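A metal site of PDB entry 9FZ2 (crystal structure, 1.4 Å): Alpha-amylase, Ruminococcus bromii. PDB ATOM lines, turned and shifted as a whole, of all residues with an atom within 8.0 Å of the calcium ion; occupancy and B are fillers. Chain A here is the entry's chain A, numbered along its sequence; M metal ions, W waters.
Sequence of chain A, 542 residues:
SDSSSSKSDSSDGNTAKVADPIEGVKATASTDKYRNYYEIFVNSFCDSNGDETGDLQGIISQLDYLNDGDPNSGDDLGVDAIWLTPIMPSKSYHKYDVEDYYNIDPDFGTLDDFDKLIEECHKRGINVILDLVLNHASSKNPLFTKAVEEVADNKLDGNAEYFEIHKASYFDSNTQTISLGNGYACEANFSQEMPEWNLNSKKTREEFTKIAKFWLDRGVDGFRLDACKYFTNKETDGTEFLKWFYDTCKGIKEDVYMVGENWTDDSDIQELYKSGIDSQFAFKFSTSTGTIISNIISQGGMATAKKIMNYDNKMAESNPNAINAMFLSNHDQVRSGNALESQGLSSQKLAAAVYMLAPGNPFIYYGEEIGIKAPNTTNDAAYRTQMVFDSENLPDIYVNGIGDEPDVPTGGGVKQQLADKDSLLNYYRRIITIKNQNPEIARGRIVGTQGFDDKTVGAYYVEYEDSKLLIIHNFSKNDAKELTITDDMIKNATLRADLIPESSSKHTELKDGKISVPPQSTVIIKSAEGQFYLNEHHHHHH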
ATOM      1  N   VAL A  42       5.181  15.766  -1.941  1.00  0.00           N
ATOM      2  CA  VAL A  42       5.642  17.074  -1.486  1.00  0.00           C
ATOM      3  C   VAL A  42       6.189  17.938  -2.630  1.00  0.00           C
ATOM      4  O   VAL A  42       5.874  19.133  -2.764  1.00  0.00           O
ATOM      5  CB  VAL A  42       6.603  16.959  -0.288  1.00  0.00           C
ATOM      6  CG1 VAL A  42       7.069  18.338   0.120  1.00  0.00           C
ATOM      7  CG2 VAL A  42       5.928  16.284   0.909  1.00  0.00           C
ATOM      8  N   ASN A  43       7.008  17.349  -3.498  1.00  0.00           N
ATOM      9  CA  ASN A  43       7.608  18.075  -4.592  1.00  0.00           C
ATOM     10  C   ASN A  43       6.556  18.849  -5.385  1.00  0.00           C
ATOM     11  O   ASN A  43       6.852  19.894  -5.923  1.00  0.00           O
ATOM     12  CB  ASN A  43       8.284  17.159  -5.590  1.00  0.00           C
ATOM     13  CG  ASN A  43       8.901  17.859  -6.776  1.00  0.00           C
ATOM     14  OD1 ASN A  43      10.022  18.303  -6.666  1.00  0.00           O
ATOM     15  ND2 ASN A  43       8.235  17.937  -7.913  1.00  0.00           N
ATOM     16  N   CYS A  46       2.937  22.505  -3.435  1.00  0.00           N
ATOM     17  CA  CYS A  46       2.888  23.965  -3.339  1.00  0.00           C
ATOM     18  C   CYS A  46       4.271  24.551  -3.086  1.00  0.00           C
ATOM     19  O   CYS A  46       4.888  24.249  -2.060  1.00  0.00           O
ATOM     20  CB  CYS A  46       1.918  24.456  -2.263  1.00  0.00           C
ATOM     21  SG  CYS A  46       1.674  26.255  -2.261  1.00  0.00           S
ATOM     22  N   ASP A  47       4.730  25.341  -4.046  1.00  0.00           N
ATOM     23  CA  ASP A  47       6.015  26.028  -3.964  1.00  0.00           C
ATOM     24  C   ASP A  47       5.812  27.409  -3.340  1.00  0.00           C
ATOM     25  O   ASP A  47       5.208  28.255  -3.990  1.00  0.00           O
ATOM     26  CB  ASP A  47       6.613  26.148  -5.365  1.00  0.00           C
ATOM     27  CG  ASP A  47       7.961  26.850  -5.419  1.00  0.00           C
ATOM     28  OD1 ASP A  47       8.593  27.004  -4.361  1.00  0.00           O
ATOM     29  OD2 ASP A  47       8.359  27.326  -6.497  1.00  0.00           O
ATOM     30  N   SER A  48       6.429  27.662  -2.188  1.00  0.00           N
ATOM     31  CA  SER A  48       6.318  28.945  -1.484  1.00  0.00           C
ATOM     32  C   SER A  48       7.480  29.912  -1.757  1.00  0.00           C
ATOM     33  O   SER A  48       7.449  31.030  -1.217  1.00  0.00           O
ATOM     34  CB  SER A  48       6.167  28.709  -0.027  1.00  0.00           C
ATOM     35  OG  SER A  48       7.381  28.222   0.523  1.00  0.00           O
ATOM     36  N   ASN A  49       8.512  29.512  -2.534  1.00  0.00           N
ATOM     37  CA  ASN A  49       9.726  30.340  -2.614  1.00  0.00           C
ATOM     38  C   ASN A  49      10.406  30.323  -3.999  1.00  0.00           C
ATOM     39  O   ASN A  49      11.587  30.663  -4.133  1.00  0.00           O
ATOM     40  CB  ASN A  49      10.697  29.987  -1.487  1.00  0.00           C
ATOM     41  CG  ASN A  49      11.197  28.583  -1.580  1.00  0.00           C
ATOM     42  OD1 ASN A  49      10.907  27.876  -2.545  1.00  0.00           O
ATOM     43  ND2 ASN A  49      12.015  28.192  -0.616  1.00  0.00           N
ATOM     44  N   GLY A  50       9.654  29.983  -5.026  1.00  0.00           N
ATOM     45  CA  GLY A  50       9.989  30.294  -6.406  1.00  0.00           C
ATOM     46  C   GLY A  50      11.040  29.434  -7.098  1.00  0.00           C
ATOM     47  O   GLY A  50      11.327  29.711  -8.263  1.00  0.00           O
ATOM     48  N   ASP A  51      11.562  28.373  -6.459  1.00  0.00           N
ATOM     49  CA  ASP A  51      12.532  27.485  -7.113  1.00  0.00           C
ATOM     50  C   ASP A  51      11.897  26.415  -8.009  1.00  0.00           C
ATOM     51  O   ASP A  51      12.630  25.661  -8.633  1.00  0.00           O
ATOM     52  CB  ASP A  51      13.444  26.833  -6.072  1.00  0.00           C
ATOM     53  CG  ASP A  51      12.764  25.864  -5.123  1.00  0.00           C
ATOM     54  OD1 ASP A  51      11.492  25.942  -5.009  1.00  0.00           O
ATOM     55  OD2 ASP A  51      13.512  25.029  -4.522  1.00  0.00           O
ATOM     56  N   GLU A  52      10.569  26.336  -8.051  1.00  0.00           N
ATOM     57  CA  GLU A  52       9.816  25.338  -8.805  1.00  0.00           C
ATOM     58  C   GLU A  52       9.816  23.987  -8.087  1.00  0.00           C
ATOM     59  O   GLU A  52       9.546  22.945  -8.689  1.00  0.00           O
ATOM     60  CB  GLU A  52      10.248  25.213 -10.260  1.00  0.00           C
ATOM     61  CG  GLU A  52      10.133  26.543 -11.018  1.00  0.00           C
ATOM     62  CD  GLU A  52      10.369  26.390 -12.509  1.00  0.00           C
ATOM     63  OE1 GLU A  52      10.082  25.303 -13.080  1.00  0.00           O
ATOM     64  OE2 GLU A  52      10.900  27.351 -13.120  1.00  0.00           O
ATOM     65  N   THR A  53      10.053  23.989  -6.770  1.00  0.00           N
ATOM     66  CA  THR A  53       9.974  22.776  -5.985  1.00  0.00           C
ATOM     67  C   THR A  53       8.962  22.992  -4.848  1.00  0.00           C
ATOM     68  O   THR A  53       9.088  23.946  -4.096  1.00  0.00           O
ATOM     69  CB  THR A  53      11.334  22.404  -5.406  1.00  0.00           C
ATOM     70  OG1 THR A  53      12.246  22.282  -6.492  1.00  0.00           O
ATOM     71  CG2 THR A  53      11.308  21.097  -4.643  1.00  0.00           C
ATOM     72  N   GLY A  54       8.002  22.086  -4.678  1.00  0.00           N
ATOM     73  CA  GLY A  54       7.081  22.207  -3.565  1.00  0.00           C
ATOM     74  C   GLY A  54       7.785  21.999  -2.225  1.00  0.00           C
ATOM     75  O   GLY A  54       8.822  21.339  -2.164  1.00  0.00           O
ATOM     76  N   ASP A  55       7.254  22.637  -1.177  1.00  0.00           N
ATOM     77  CA  ASP A  55       7.955  22.689   0.087  1.00  0.00           C
ATOM     78  C   ASP A  55       6.944  22.688   1.241  1.00  0.00           C
ATOM     79  O   ASP A  55       5.744  22.695   1.005  1.00  0.00           O
ATOM     80  CB  ASP A  55       8.913  23.866   0.132  1.00  0.00           C
ATOM     81  CG  ASP A  55       8.274  25.190  -0.242  1.00  0.00           C
ATOM     82  OD1 ASP A  55       7.352  25.572   0.497  1.00  0.00           O
ATOM     83  OD2 ASP A  55       8.624  25.744  -1.296  1.00  0.00           O
ATOM     84  N   LEU A  56       7.451  22.532   2.480  1.00  0.00           N
ATOM     85  CA  LEU A  56       6.577  22.491   3.656  1.00  0.00           C
ATOM     86  C   LEU A  56       5.826  23.809   3.894  1.00  0.00           C
ATOM     87  O   LEU A  56       4.630  23.784   4.248  1.00  0.00           O
ATOM     88  CB  LEU A  56       7.352  22.080   4.911  1.00  0.00           C
ATOM     89  CG  LEU A  56       8.097  20.740   4.820  1.00  0.00           C
ATOM     90  CD1 LEU A  56       8.740  20.427   6.152  1.00  0.00           C
ATOM     91  CD2 LEU A  56       7.180  19.612   4.380  1.00  0.00           C
ATOM     92  N   GLN A  57       6.468  24.959   3.698  1.00  0.00           N
ATOM     93  CA  GLN A  57       5.776  26.251   3.829  1.00  0.00           C
ATOM     94  C   GLN A  57       4.646  26.371   2.828  1.00  0.00           C
ATOM     95  O   GLN A  57       3.603  26.908   3.157  1.00  0.00           O
ATOM     96  CB  GLN A  57       6.709  27.466   3.843  1.00  0.00           C
ATOM     97  CG  GLN A  57       7.463  27.605   5.157  1.00  0.00           C
ATOM     98  CD  GLN A  57       6.624  28.078   6.329  1.00  0.00           C
ATOM     99  OE1 GLN A  57       5.460  28.498   6.189  1.00  0.00           O
ATOM    100  NE2 GLN A  57       7.220  27.987   7.510  1.00  0.00           N
ATOM    101  N   GLY A  58       4.820  25.768   1.648  1.00  0.00           N
ATOM    102  CA  GLY A  58       3.748  25.739   0.678  1.00  0.00           C
ATOM    103  C   GLY A  58       2.549  24.949   1.189  1.00  0.00           C
ATOM    104  O   GLY A  58       1.408  25.409   1.074  1.00  0.00           O
ATOM    105  N   PRO A 106      16.695  20.169   2.478  1.00  0.00           N
ATOM    106  CA  PRO A 106      16.755  21.640   2.431  1.00  0.00           C
ATOM    107  C   PRO A 106      15.768  22.299   1.470  1.00  0.00           C
ATOM    108  O   PRO A 106      15.286  23.402   1.755  1.00  0.00           O
ATOM    109  CB  PRO A 106      18.218  21.882   2.009  1.00  0.00           C
ATOM    110  CG  PRO A 106      18.936  20.761   2.637  1.00  0.00           C
ATOM    111  CD  PRO A 106      18.042  19.567   2.345  1.00  0.00           C
ATOM    112  N   ASP A 107      15.458  21.606   0.364  1.00  0.00           N
ATOM    113  CA  ASP A 107      14.473  22.129  -0.562  1.00  0.00           C
ATOM    114  C   ASP A 107      13.095  22.204   0.091  1.00  0.00           C
ATOM    115  O   ASP A 107      12.310  23.065  -0.269  1.00  0.00           O
ATOM    116  CB  ASP A 107      14.388  21.293  -1.828  1.00  0.00           C
ATOM    117  CG  ASP A 107      15.468  21.554  -2.870  1.00  0.00           C
ATOM    118  OD1 ASP A 107      16.134  22.618  -2.799  1.00  0.00           O
ATOM    119  OD2 ASP A 107      15.560  20.682  -3.756  1.00  0.00           O
ATOM    120  N   PHE A 108      12.789  21.297   1.039  1.00  0.00           N
ATOM    121  CA  PHE A 108      11.472  21.299   1.665  1.00  0.00           C
ATOM    122  C   PHE A 108      11.401  22.267   2.845  1.00  0.00           C
ATOM    123  O   PHE A 108      10.296  22.677   3.202  1.00  0.00           O
ATOM    124  CB  PHE A 108      11.060  19.872   2.058  1.00  0.00           C
ATOM    125  CG  PHE A 108      10.840  18.946   0.880  1.00  0.00           C
ATOM    126  CD1 PHE A 108      10.728  19.384  -0.444  1.00  0.00           C
ATOM    127  CD2 PHE A 108      10.651  17.602   1.125  1.00  0.00           C
ATOM    128  CE1 PHE A 108      10.512  18.470  -1.487  1.00  0.00           C
ATOM    129  CE2 PHE A 108      10.429  16.724   0.103  1.00  0.00           C
ATOM    130  CZ  PHE A 108      10.353  17.156  -1.201  1.00  0.00           C
ATOM    131  N   GLY A 109      12.550  22.625   3.447  1.00  0.00           N
ATOM    132  CA  GLY A 109      12.545  23.520   4.586  1.00  0.00           C
ATOM    133  C   GLY A 109      13.480  22.969   5.660  1.00  0.00           C
ATOM    134  O   GLY A 109      14.455  22.273   5.356  1.00  0.00           O
ATOM    135  N   ASP A 396       3.977  26.645 -11.318  1.00  0.00           N
ATOM    136  CA  ASP A 396       5.294  26.684 -11.958  1.00  0.00           C
ATOM    137  C   ASP A 396       6.178  25.778 -11.112  1.00  0.00           C
ATOM    138  O   ASP A 396       6.931  26.238 -10.260  1.00  0.00           O
ATOM    139  CB  ASP A 396       5.742  28.130 -12.092  1.00  0.00           C
ATOM    140  CG  ASP A 396       7.027  28.363 -12.858  1.00  0.00           C
ATOM    141  OD1 ASP A 396       7.471  27.419 -13.509  1.00  0.00           O
ATOM    142  OD2 ASP A 396       7.510  29.488 -12.817  1.00  0.00           O
ATOM    143  N   ILE A 397       5.974  24.471 -11.259  1.00  0.00           N
ATOM    144  CA  ILE A 397       6.699  23.467 -10.476  1.00  0.00           C
ATOM    145  C   ILE A 397       7.314  22.490 -11.459  1.00  0.00           C
ATOM    146  O   ILE A 397       6.690  22.085 -12.438  1.00  0.00           O
ATOM    147  CB  ILE A 397       5.804  22.753  -9.443  1.00  0.00           C
ATOM    148  CG1 ILE A 397       5.614  23.628  -8.209  1.00  0.00           C
ATOM    149  CG2 ILE A 397       6.363  21.381  -9.053  1.00  0.00           C
ATOM    150  CD1 ILE A 397       4.779  23.044  -7.071  1.00  0.00           C
HETATM  151 CA    CA M   1      10.084  25.807  -3.134  1.00  0.00          CA
HETATM  152  O   HOH W   1      12.078  24.620  -2.245  1.00  0.00           O
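Within 4 Å of the calcium ion: Asp 47, Asn 49, Asp 51, Thr 53 and Asp 55. The nearest printed residue that does not touch the calcium ion is Ser 48 (4.2 Å).
The backbone NH of Gly 50 lies within hydrogen-bond range of the side-chain carboxylate of Asp 47 (3.3 Å). N of Glu 52 lies within hydrogen-bond range of OD2 of Asp 47 (2.9 Å). The side-chain carboxylate (OD1) of Asp 55 sits at hydrogen-bond distance from the side-chain hydroxyl (OG) of Ser 48 (2.7 Å). The backbone carbonyl oxygen (O) of Cys 46 is in hydrogen-bond range of the backbone NH (N) of Asp 55 (3.0 Å). N of Gly 58 is in hydrogen-bond range of OD1 of Asp 55 (2.8 Å). N of Gln 57 lies within hydrogen-bond range of OD1 of Asp 55.
Water W1 bridges the backbone carbonyl oxygen (O) of Asp 107 (2.5 Å) and the side-chain carboxylate (OD2) of Asp 51 (2.7 Å).
The calcium ion is bound by the side-chain carboxylate of Asp 47 (2.3 Å), the side-chain amide oxygen of Asn 49 (2.3 Å), the backbone carbonyl oxygen of Thr 53 (2.3 Å), the side-chain carboxylate of Asp 55 (2.3 Å), the side-chain carboxylate of Asp 51 (2.3 Å) and water W1 (2.5 Å).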
